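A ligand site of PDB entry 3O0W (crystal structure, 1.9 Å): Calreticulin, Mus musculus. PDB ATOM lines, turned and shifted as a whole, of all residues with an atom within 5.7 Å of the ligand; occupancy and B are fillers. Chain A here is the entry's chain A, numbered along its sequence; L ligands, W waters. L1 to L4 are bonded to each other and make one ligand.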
ATOM      1  N   PHE A  60      15.274 -13.427   4.860  1.00  0.00           N
ATOM      2  CA  PHE A  60      15.858 -12.175   5.332  1.00  0.00           C
ATOM      3  C   PHE A  60      16.369 -12.391   6.749  1.00  0.00           C
ATOM      4  O   PHE A  60      15.775 -13.128   7.527  1.00  0.00           O
ATOM      5  CB  PHE A  60      14.844 -11.035   5.313  1.00  0.00           C
ATOM      6  CG  PHE A  60      14.604 -10.468   3.948  1.00  0.00           C
ATOM      7  CD1 PHE A  60      15.510  -9.582   3.383  1.00  0.00           C
ATOM      8  CD2 PHE A  60      13.475 -10.833   3.222  1.00  0.00           C
ATOM      9  CE1 PHE A  60      15.292  -9.051   2.101  1.00  0.00           C
ATOM     10  CE2 PHE A  60      13.259 -10.311   1.937  1.00  0.00           C
ATOM     11  CZ  PHE A  60      14.164  -9.420   1.388  1.00  0.00           C
ATOM     12  N   TYR A  61      17.463 -11.705   7.074  1.00  0.00           N
ATOM     13  CA  TYR A  61      18.128 -11.809   8.369  1.00  0.00           C
ATOM     14  C   TYR A  61      18.229 -10.413   8.974  1.00  0.00           C
ATOM     15  O   TYR A  61      18.512  -9.447   8.264  1.00  0.00           O
ATOM     16  CB  TYR A  61      19.513 -12.448   8.212  1.00  0.00           C
ATOM     17  CG  TYR A  61      19.461 -13.947   7.956  1.00  0.00           C
ATOM     18  CD1 TYR A  61      19.336 -14.459   6.666  1.00  0.00           C
ATOM     19  CD2 TYR A  61      19.527 -14.849   9.019  1.00  0.00           C
ATOM     20  CE1 TYR A  61      19.270 -15.840   6.436  1.00  0.00           C
ATOM     21  CE2 TYR A  61      19.470 -16.235   8.808  1.00  0.00           C
ATOM     22  CZ  TYR A  61      19.329 -16.714   7.509  1.00  0.00           C
ATOM     23  OH  TYR A  61      19.266 -18.072   7.308  1.00  0.00           O
ATOM     24  N   CYS A  91      23.582 -16.509  -4.189  1.00  0.00           N
ATOM     25  CA  CYS A  91      23.105 -15.154  -3.970  1.00  0.00           C
ATOM     26  C   CYS A  91      22.966 -14.956  -2.465  1.00  0.00           C
ATOM     27  O   CYS A  91      22.330 -15.756  -1.784  1.00  0.00           O
ATOM     28  CB  CYS A  91      21.762 -14.938  -4.663  1.00  0.00           C
ATOM     29  SG  CYS A  91      20.990 -13.358  -4.266  1.00  0.00           S
ATOM     30  N   GLY A  92      23.561 -13.905  -1.940  1.00  0.00           N
ATOM     31  CA  GLY A  92      23.398 -13.583  -0.527  1.00  0.00           C
ATOM     32  C   GLY A  92      24.357 -12.513  -0.086  1.00  0.00           C
ATOM     33  O   GLY A  92      25.492 -12.444  -0.592  1.00  0.00           O
ATOM     34  N   GLY A  93      23.912 -11.670   0.847  1.00  0.00           N
ATOM     35  CA  GLY A  93      24.747 -10.586   1.378  1.00  0.00           C
ATOM     36  C   GLY A  93      25.757 -11.068   2.409  1.00  0.00           C
ATOM     37  O   GLY A  93      25.614 -12.163   2.966  1.00  0.00           O
ATOM     38  N   TYR A  95      27.578  -8.234   4.289  1.00  0.00           N
ATOM     39  CA  TYR A  95      27.982  -6.895   4.703  1.00  0.00           C
ATOM     40  C   TYR A  95      27.331  -6.491   6.027  1.00  0.00           C
ATOM     41  O   TYR A  95      26.336  -7.097   6.450  1.00  0.00           O
ATOM     42  CB  TYR A  95      27.642  -5.876   3.621  1.00  0.00           C
ATOM     43  CG  TYR A  95      26.224  -5.984   3.081  1.00  0.00           C
ATOM     44  CD1 TYR A  95      25.962  -6.699   1.903  1.00  0.00           C
ATOM     45  CD2 TYR A  95      25.150  -5.377   3.745  1.00  0.00           C
ATOM     46  CE1 TYR A  95      24.661  -6.800   1.393  1.00  0.00           C
ATOM     47  CE2 TYR A  95      23.843  -5.483   3.243  1.00  0.00           C
ATOM     48  CZ  TYR A  95      23.614  -6.182   2.072  1.00  0.00           C
ATOM     49  OH  TYR A  95      22.329  -6.289   1.558  1.00  0.00           O
ATOM     50  N   LYS A  97      26.041  -3.094   8.684  1.00  0.00           N
ATOM     51  CA  LYS A  97      25.610  -1.701   8.737  1.00  0.00           C
ATOM     52  C   LYS A  97      25.962  -1.145  10.113  1.00  0.00           C
ATOM     53  O   LYS A  97      25.894  -1.850  11.117  1.00  0.00           O
ATOM     54  CB  LYS A  97      24.105  -1.599   8.496  1.00  0.00           C
ATOM     55  CG  LYS A  97      23.647  -1.769   7.036  1.00  0.00           C
ATOM     56  CD  LYS A  97      22.128  -1.685   6.957  1.00  0.00           C
ATOM     57  CE  LYS A  97      21.625  -1.506   5.527  1.00  0.00           C
ATOM     58  NZ  LYS A  97      20.140  -1.735   5.401  1.00  0.00           N
ATOM     59  N   HIS A 109      15.286  -3.239  10.223  1.00  0.00           N
ATOM     60  CA  HIS A 109      15.051  -3.913   8.949  1.00  0.00           C
ATOM     61  C   HIS A 109      15.874  -3.229   7.864  1.00  0.00           C
ATOM     62  O   HIS A 109      16.644  -2.315   8.161  1.00  0.00           O
ATOM     63  CB  HIS A 109      13.545  -3.916   8.606  1.00  0.00           C
ATOM     64  CG  HIS A 109      12.937  -2.549   8.526  1.00  0.00           C
ATOM     65  ND1 HIS A 109      12.585  -1.826   9.640  1.00  0.00           N
ATOM     66  CD2 HIS A 109      12.607  -1.787   7.464  1.00  0.00           C
ATOM     67  CE1 HIS A 109      12.062  -0.659   9.263  1.00  0.00           C
ATOM     68  NE2 HIS A 109      12.070  -0.615   7.940  1.00  0.00           N
ATOM     69  N   GLY A 110      15.691  -3.672   6.620  1.00  0.00           N
ATOM     70  CA  GLY A 110      16.481  -3.184   5.483  1.00  0.00           C
ATOM     71  C   GLY A 110      16.429  -1.684   5.244  1.00  0.00           C
ATOM     72  O   GLY A 110      17.385  -1.096   4.724  1.00  0.00           O
ATOM     73  N   ASP A 111      15.317  -1.058   5.619  1.00  0.00           N
ATOM     74  CA  ASP A 111      15.128   0.375   5.386  1.00  0.00           C
ATOM     75  C   ASP A 111      15.334   1.266   6.615  1.00  0.00           C
ATOM     76  O   ASP A 111      15.147   2.478   6.542  1.00  0.00           O
ATOM     77  CB  ASP A 111      13.751   0.621   4.738  1.00  0.00           C
ATOM     78  CG  ASP A 111      13.580  -0.143   3.425  1.00  0.00           C
ATOM     79  OD1 ASP A 111      14.519  -0.125   2.602  1.00  0.00           O
ATOM     80  OD2 ASP A 111      12.502  -0.773   3.228  1.00  0.00           O
ATOM     81  N   TYR A 114      20.715   4.038   8.521  1.00  0.00           N
ATOM     82  CA  TYR A 114      22.079   3.671   8.921  1.00  0.00           C
ATOM     83  C   TYR A 114      23.079   4.765   8.507  1.00  0.00           C
ATOM     84  O   TYR A 114      22.752   5.600   7.670  1.00  0.00           O
ATOM     85  CB  TYR A 114      22.467   2.332   8.299  1.00  0.00           C
ATOM     86  CG  TYR A 114      22.476   2.300   6.793  1.00  0.00           C
ATOM     87  CD1 TYR A 114      21.312   1.983   6.065  1.00  0.00           C
ATOM     88  CD2 TYR A 114      23.642   2.565   6.069  1.00  0.00           C
ATOM     89  CE1 TYR A 114      21.320   1.949   4.656  1.00  0.00           C
ATOM     90  CE2 TYR A 114      23.656   2.540   4.670  1.00  0.00           C
ATOM     91  CZ  TYR A 114      22.494   2.223   3.972  1.00  0.00           C
ATOM     92  OH  TYR A 114      22.507   2.202   2.589  1.00  0.00           O
ATOM     93  N   MET A 117      27.283   1.399   5.408  1.00  0.00           N
ATOM     94  CA  MET A 117      27.159  -0.017   5.054  1.00  0.00           C
ATOM     95  C   MET A 117      28.416  -0.445   4.316  1.00  0.00           C
ATOM     96  O   MET A 117      28.839   0.202   3.346  1.00  0.00           O
ATOM     97  CB  MET A 117      25.897  -0.262   4.214  1.00  0.00           C
ATOM     98  CG  MET A 117      25.778  -1.665   3.647  1.00  0.00           C
ATOM     99  SD  MET A 117      24.118  -1.936   2.677  1.00  0.00           S
ATOM    100  CE  MET A 117      24.850  -2.900   1.150  1.00  0.00           C
ATOM    101  N   ASP A 121      28.889  -8.397  -1.252  1.00  0.00           N
ATOM    102  CA  ASP A 121      27.537  -8.758  -1.651  1.00  0.00           C
ATOM    103  C   ASP A 121      27.698  -9.624  -2.889  1.00  0.00           C
ATOM    104  O   ASP A 121      28.567  -9.368  -3.722  1.00  0.00           O
ATOM    105  CB  ASP A 121      26.729  -7.494  -1.969  1.00  0.00           C
ATOM    106  CG  ASP A 121      25.235  -7.777  -2.104  1.00  0.00           C
ATOM    107  OD1 ASP A 121      24.779  -8.849  -1.665  1.00  0.00           O
ATOM    108  OD2 ASP A 121      24.514  -6.905  -2.637  1.00  0.00           O
ATOM    109  N   ILE A 122      26.880 -10.673  -2.990  1.00  0.00           N
ATOM    110  CA  ILE A 122      26.938 -11.597  -4.134  1.00  0.00           C
ATOM    111  C   ILE A 122      25.521 -11.914  -4.576  1.00  0.00           C
ATOM    112  O   ILE A 122      24.649 -12.214  -3.742  1.00  0.00           O
ATOM    113  CB  ILE A 122      27.710 -12.911  -3.790  1.00  0.00           C
ATOM    114  CG1 ILE A 122      29.144 -12.605  -3.338  1.00  0.00           C
ATOM    115  CG2 ILE A 122      27.712 -13.891  -4.996  1.00  0.00           C
ATOM    116  CD1 ILE A 122      29.958 -13.808  -2.911  1.00  0.00           C
ATOM    117  N   CYS A 123      25.264 -11.802  -5.869  1.00  0.00           N
ATOM    118  CA  CYS A 123      23.953 -12.150  -6.397  1.00  0.00           C
ATOM    119  C   CYS A 123      24.081 -12.569  -7.837  1.00  0.00           C
ATOM    120  O   CYS A 123      23.937 -11.758  -8.760  1.00  0.00           O
ATOM    121  CB  CYS A 123      22.967 -10.995  -6.258  1.00  0.00           C
ATOM    122  SG  CYS A 123      21.279 -11.562  -6.457  1.00  0.00           S
ATOM    123  N   THR A 127      26.745  -9.703  -9.871  1.00  0.00           N
ATOM    124  CA  THR A 127      26.985  -8.972  -8.632  1.00  0.00           C
ATOM    125  C   THR A 127      27.984  -9.707  -7.750  1.00  0.00           C
ATOM    126  O   THR A 127      27.668 -10.736  -7.130  1.00  0.00           O
ATOM    127  CB  THR A 127      25.663  -8.736  -7.857  1.00  0.00           C
ATOM    128  OG1 THR A 127      24.755  -8.006  -8.694  1.00  0.00           O
ATOM    129  CG2 THR A 127      25.899  -7.950  -6.561  1.00  0.00           C
ATOM    130  N   HIS A 131      30.431  -3.430  -1.182  1.00  0.00           N
ATOM    131  CA  HIS A 131      29.739  -2.172  -0.955  1.00  0.00           C
ATOM    132  C   HIS A 131      30.488  -1.292   0.025  1.00  0.00           C
ATOM    133  O   HIS A 131      31.039  -1.793   1.019  1.00  0.00           O
ATOM    134  CB  HIS A 131      28.320  -2.410  -0.411  1.00  0.00           C
ATOM    135  CG  HIS A 131      27.310  -2.722  -1.475  1.00  0.00           C
ATOM    136  ND1 HIS A 131      26.925  -1.805  -2.426  1.00  0.00           N
ATOM    137  CD2 HIS A 131      26.580  -3.834  -1.707  1.00  0.00           C
ATOM    138  CE1 HIS A 131      26.021  -2.352  -3.222  1.00  0.00           C
ATOM    139  NE2 HIS A 131      25.788  -3.583  -2.801  1.00  0.00           N
ATOM    140  N   ILE A 133      29.033   2.275   1.470  1.00  0.00           N
ATOM    141  CA  ILE A 133      27.949   3.248   1.384  1.00  0.00           C
ATOM    142  C   ILE A 133      28.002   4.206   2.567  1.00  0.00           C
ATOM    143  O   ILE A 133      28.078   3.772   3.728  1.00  0.00           O
ATOM    144  CB  ILE A 133      26.565   2.551   1.293  1.00  0.00           C
ATOM    145  CG1 ILE A 133      26.552   1.506   0.165  1.00  0.00           C
ATOM    146  CG2 ILE A 133      25.447   3.568   1.091  1.00  0.00           C
ATOM    147  CD1 ILE A 133      25.265   0.695   0.091  1.00  0.00           C
ATOM    148  N   ASN A 140      21.732   7.516   0.755  1.00  0.00           N
ATOM    149  CA  ASN A 140      22.764   6.513   0.922  1.00  0.00           C
ATOM    150  C   ASN A 140      23.589   6.381  -0.346  1.00  0.00           C
ATOM    151  O   ASN A 140      23.114   5.824  -1.345  1.00  0.00           O
ATOM    152  CB  ASN A 140      22.141   5.169   1.312  1.00  0.00           C
ATOM    153  CG  ASN A 140      21.298   5.257   2.568  1.00  0.00           C
ATOM    154  OD1 ASN A 140      21.717   5.837   3.590  1.00  0.00           O
ATOM    155  ND2 ASN A 140      20.077   4.697   2.506  1.00  0.00           N
ATOM    156  N   LEU A 142      26.561   5.210  -2.819  1.00  0.00           N
ATOM    157  CA  LEU A 142      27.428   4.078  -3.128  1.00  0.00           C
ATOM    158  C   LEU A 142      28.743   4.522  -3.770  1.00  0.00           C
ATOM    159  O   LEU A 142      28.764   5.422  -4.621  1.00  0.00           O
ATOM    160  CB  LEU A 142      26.703   3.090  -4.064  1.00  0.00           C
ATOM    161  CG  LEU A 142      25.616   2.135  -3.517  1.00  0.00           C
ATOM    162  CD1 LEU A 142      24.391   2.892  -3.007  1.00  0.00           C
ATOM    163  CD2 LEU A 142      25.190   1.119  -4.574  1.00  0.00           C
ATOM    164  N   ASP A 214      21.932  -7.142   8.248  1.00  0.00           N
ATOM    165  CA  ASP A 214      20.691  -7.060   7.481  1.00  0.00           C
ATOM    166  C   ASP A 214      21.002  -7.710   6.135  1.00  0.00           C
ATOM    167  O   ASP A 214      21.618  -7.079   5.273  1.00  0.00           O
ATOM    168  CB  ASP A 214      20.276  -5.588   7.294  1.00  0.00           C
ATOM    169  CG  ASP A 214      19.380  -5.386   6.088  1.00  0.00           C
ATOM    170  OD1 ASP A 214      18.416  -6.172   5.914  1.00  0.00           O
ATOM    171  OD2 ASP A 214      19.644  -4.452   5.302  1.00  0.00           O
ATOM    172  N   LEU A 215      20.575  -8.958   5.964  1.00  0.00           N
ATOM    173  CA  LEU A 215      20.922  -9.741   4.771  1.00  0.00           C
ATOM    174  C   LEU A 215      19.714 -10.398   4.141  1.00  0.00           C
ATOM    175  O   LEU A 215      18.707 -10.671   4.809  1.00  0.00           O
ATOM    176  CB  LEU A 215      21.921 -10.850   5.148  1.00  0.00           C
ATOM    177  CG  LEU A 215      23.114 -10.464   6.037  1.00  0.00           C
ATOM    178  CD1 LEU A 215      23.776 -11.689   6.636  1.00  0.00           C
ATOM    179  CD2 LEU A 215      24.148  -9.577   5.310  1.00  0.00           C
ATOM    180  N   TRP A 216      19.837 -10.627   2.832  1.00  0.00           N
ATOM    181  CA  TRP A 216      19.049 -11.628   2.134  1.00  0.00           C
ATOM    182  C   TRP A 216      20.010 -12.716   1.645  1.00  0.00           C
ATOM    183  O   TRP A 216      21.118 -12.416   1.174  1.00  0.00           O
ATOM    184  CB  TRP A 216      18.305 -11.024   0.938  1.00  0.00           C
ATOM    185  CG  TRP A 216      17.750 -12.077  -0.007  1.00  0.00           C
ATOM    186  CD1 TRP A 216      18.320 -12.525  -1.168  1.00  0.00           C
ATOM    187  CD2 TRP A 216      16.559 -12.858   0.170  1.00  0.00           C
ATOM    188  NE1 TRP A 216      17.549 -13.503  -1.741  1.00  0.00           N
ATOM    189  CE2 TRP A 216      16.468 -13.735  -0.929  1.00  0.00           C
ATOM    190  CE3 TRP A 216      15.562 -12.895   1.161  1.00  0.00           C
ATOM    191  CZ2 TRP A 216      15.404 -14.639  -1.082  1.00  0.00           C
ATOM    192  CZ3 TRP A 216      14.499 -13.799   1.008  1.00  0.00           C
ATOM    193  CH2 TRP A 216      14.429 -14.652  -0.116  1.00  0.00           C
ATOM    194  N   VAL A 218      19.831 -16.632  -0.567  1.00  0.00           N
ATOM    195  CA  VAL A 218      19.198 -17.808  -1.165  1.00  0.00           C
ATOM    196  C   VAL A 218      19.832 -19.011  -0.464  1.00  0.00           C
ATOM    197  O   VAL A 218      19.265 -19.526   0.503  1.00  0.00           O
ATOM    198  CB  VAL A 218      19.364 -17.833  -2.707  1.00  0.00           C
ATOM    199  CG1 VAL A 218      18.803 -19.121  -3.307  1.00  0.00           C
ATOM    200  CG2 VAL A 218      18.658 -16.619  -3.334  1.00  0.00           C
HETATM  201  C1  LIG L   1      17.748 -10.384  -5.515  1.00  0.00           C
HETATM  202  C2  LIG L   1      17.233  -9.785  -4.252  1.00  0.00           C
HETATM  203  C3  LIG L   1      15.861 -10.171  -3.808  1.00  0.00           C
HETATM  204  C4  LIG L   1      15.089  -9.397  -4.861  1.00  0.00           C
HETATM  205  C5  LIG L   1      15.514  -9.880  -6.261  1.00  0.00           C
HETATM  206  C6  LIG L   1      14.718  -9.153  -7.318  1.00  0.00           C
HETATM  207  O1  LIG L   1      17.553 -11.793  -5.570  1.00  0.00           O
HETATM  208  O2  LIG L   1      18.028  -8.690  -3.750  1.00  0.00           O
HETATM  209  O3  LIG L   1      15.494  -9.707  -2.499  1.00  0.00           O
HETATM  210  O4  LIG L   1      13.670  -9.525  -4.679  1.00  0.00           O
HETATM  211  O5  LIG L   1      16.925  -9.734  -6.496  1.00  0.00           O
HETATM  212  O6  LIG L   1      15.584  -8.382  -8.163  1.00  0.00           O
HETATM  213  C1  LG2 L   2      18.411  -8.486  -2.403  1.00  0.00           C
HETATM  214  C2  LG2 L   2      18.910  -7.037  -2.470  1.00  0.00           C
HETATM  215  C3  LG2 L   2      20.157  -6.925  -3.353  1.00  0.00           C
HETATM  216  C4  LG2 L   2      21.226  -7.926  -2.928  1.00  0.00           C
HETATM  217  C5  LG2 L   2      20.648  -9.346  -2.840  1.00  0.00           C
HETATM  218  C6  LG2 L   2      21.645 -10.339  -2.245  1.00  0.00           C
HETATM  219  O1  LG2 L   2      19.170  -6.535  -1.158  1.00  0.00           O
HETATM  220  O2  LG2 L   2      20.725  -5.609  -3.338  1.00  0.00           O
HETATM  221  O3  LG2 L   2      22.325  -7.876  -3.855  1.00  0.00           O
HETATM  222  O4  LG2 L   2      19.468  -9.366  -2.019  1.00  0.00           O
HETATM  223  O5  LG2 L   2      22.305  -9.786  -1.110  1.00  0.00           O
HETATM  224  C1  LG3 L   3      18.045  -5.939  -0.527  1.00  0.00           C
HETATM  225  C2  LG3 L   3      18.326  -4.456  -0.318  1.00  0.00           C
HETATM  226  C3  LG3 L   3      19.472  -4.235   0.667  1.00  0.00           C
HETATM  227  C4  LG3 L   3      19.220  -5.012   1.960  1.00  0.00           C
HETATM  228  C5  LG3 L   3      18.882  -6.488   1.664  1.00  0.00           C
HETATM  229  C6  LG3 L   3      18.461  -7.245   2.913  1.00  0.00           C
HETATM  230  O1  LG3 L   3      17.135  -3.831   0.189  1.00  0.00           O
HETATM  231  O2  LG3 L   3      19.542  -2.832   0.926  1.00  0.00           O
HETATM  232  O3  LG3 L   3      20.368  -4.911   2.823  1.00  0.00           O
HETATM  233  O4  LG3 L   3      17.817  -6.593   0.713  1.00  0.00           O
HETATM  234  O5  LG3 L   3      17.378  -6.580   3.560  1.00  0.00           O
HETATM  235  C1  LG4 L   4      20.846  -2.296   1.171  1.00  0.00           C
HETATM  236  C2  LG4 L   4      20.721  -0.876   1.773  1.00  0.00           C
HETATM  237  C3  LG4 L   4      20.346   0.140   0.703  1.00  0.00           C
HETATM  238  C4  LG4 L   4      21.362   0.044  -0.417  1.00  0.00           C
HETATM  239  C5  LG4 L   4      21.375  -1.364  -1.006  1.00  0.00           C
HETATM  240  C6  LG4 L   4      22.422  -1.467  -2.117  1.00  0.00           C
HETATM  241  O1  LG4 L   4      19.741  -0.883   2.809  1.00  0.00           O
HETATM  242  O2  LG4 L   4      20.379   1.471   1.229  1.00  0.00           O
HETATM  243  O3  LG4 L   4      21.042   0.972  -1.449  1.00  0.00           O
HETATM  244  O4  LG4 L   4      21.674  -2.332   0.001  1.00  0.00           O
HETATM  245  O5  LG4 L   4      22.395  -2.811  -2.604  1.00  0.00           O
HETATM  246  O   HOH W   1      21.363   3.759  -2.203  1.00  0.00           O
HETATM  247  O   HOH W   2      15.519  -5.131   2.069  1.00  0.00           O
HETATM  248  O   HOH W   3      19.556  -2.933  -4.156  1.00  0.00           O
HETATM  249  O   HOH W   4      13.813 -11.624  -1.637  1.00  0.00           O
HETATM  250  O   HOH W   5      22.529  -5.226  -1.226  1.00  0.00           O
HETATM  251  O   HOH W   6      17.007  -1.359   1.825  1.00  0.00           O
HETATM  252  O   HOH W   7      21.898  -8.980   1.428  1.00  0.00           O
HETATM  253  O   HOH W   8      17.897 -12.176  -8.419  1.00  0.00           O
HETATM  254  O   HOH W   9      14.972  -7.214  -2.052  1.00  0.00           O
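Water W7 lies within hydrogen-bond range of O5 of LG2 L2, OH of Tyr 95, N of Trp 216 and N of Gly 93.
Water W5 lies within hydrogen-bond range of O5 of LG4 L4, OD2 of Asp 121 and OH of Tyr 95.
Water W1 bridges the backbone carbonyl oxygen of Asn 140 (2.8 Å) and an oxygen (O3) of LG4 L4 (2.9 Å).
Water W6 lies within hydrogen-bond range of OD1 of Asp 111, O of Gly 110 and O1 of LG4 L4.
The side-chain amino group (NZ) of Lys 97 is in salt-bridge range of the side-chain carboxylate (OD2) of Asp 214 (2.8 Å).
The side-chain amide nitrogen (ND2) of Asn 140 lies close to the side-chain hydroxyl (OH) of Tyr 114, 3.5 Å away.
The side-chain amino group of Lys 97 lies within hydrogen-bond range of the backbone carbonyl oxygen of Gly 110.
The backbone NH (N) of Gly 93 sits at hydrogen-bond distance from the backbone carbonyl oxygen (O) of Trp 216, 2.9 Å away.
The backbone carbonyl oxygen of Met 117 is in hydrogen-bond range of the backbone NH of Ile 133 (2.8 Å).
O of Ile 122 is in hydrogen-bond range of N of Gly 92 (2.7 Å).
The backbone NH (N) of Tyr 61 is in hydrogen-bond range of the backbone carbonyl oxygen (O) of Leu 215 (2.8 Å).
The backbone carbonyl oxygen of Cys 91 is in hydrogen-bond range of the backbone NH of Val 218 (2.9 Å).
O5 of LG3 L3 is in hydrogen-bond range of OD1 of Asp 214, 2.6 Å away.
OH of Tyr 114 is in hydrogen-bond range of O2 of LG4 L4 (2.6 Å).
The side-chain carboxylate of Asp 121 sits at hydrogen-bond distance from an oxygen (O3) of LG2 L2 (2.7 Å).
The side-chain hydroxyl (OH) of Tyr 95 sits at hydrogen-bond distance from an oxygen (O3) of LG3 L3, 2.7 Å away.
The side-chain amino group (NZ) of Lys 97 is in hydrogen-bond range of an oxygen (O1) of LG4 L4.
An oxygen (O1) of LG4 L4 is in hydrogen-bond range of the backbone carbonyl oxygen (O) of Gly 110 (3.0 Å).
The backbone NH (N) of Gly 93 is in hydrogen-bond range of an oxygen (O5) of LG2 L2.
An oxygen (O2) of LG4 L4 lies within hydrogen-bond range of the side-chain amide nitrogen (ND2) of Asn 140 (3.5 Å).
A ring nitrogen (NE2) of His 131 lies within hydrogen-bond range of an oxygen (O5) of LG4 L4 (3.5 Å).
The side-chain sulfur of Met 117 sits close to an oxygen (O4) of LG4 L4 (3.6 Å).
Residues that only touch the ligand: Trp 216, Phe 60, Gly 92, Leu 215, Cys 91, Cys 123, Ile 122 and Ile 133.
Hydrophobic or aromatic side chains that line the ligand: Phe 60, Tyr 95, Tyr 114, Met 117, His 131, Ile 133 and Trp 216.
18 residues have an atom within 4 Å of the ligand: Phe 60, Cys 91, Gly 92, Gly 93, Tyr 95, Lys 97, Gly 110, Tyr 114, Met 117, Asp 121, Ile 122, Cys 123, His 131, Ile 133, Asn 140, Asp 214, Leu 215 and Trp 216.
The nearest printed residue that does not touch the ligand is Leu 142 (4.2 Å).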
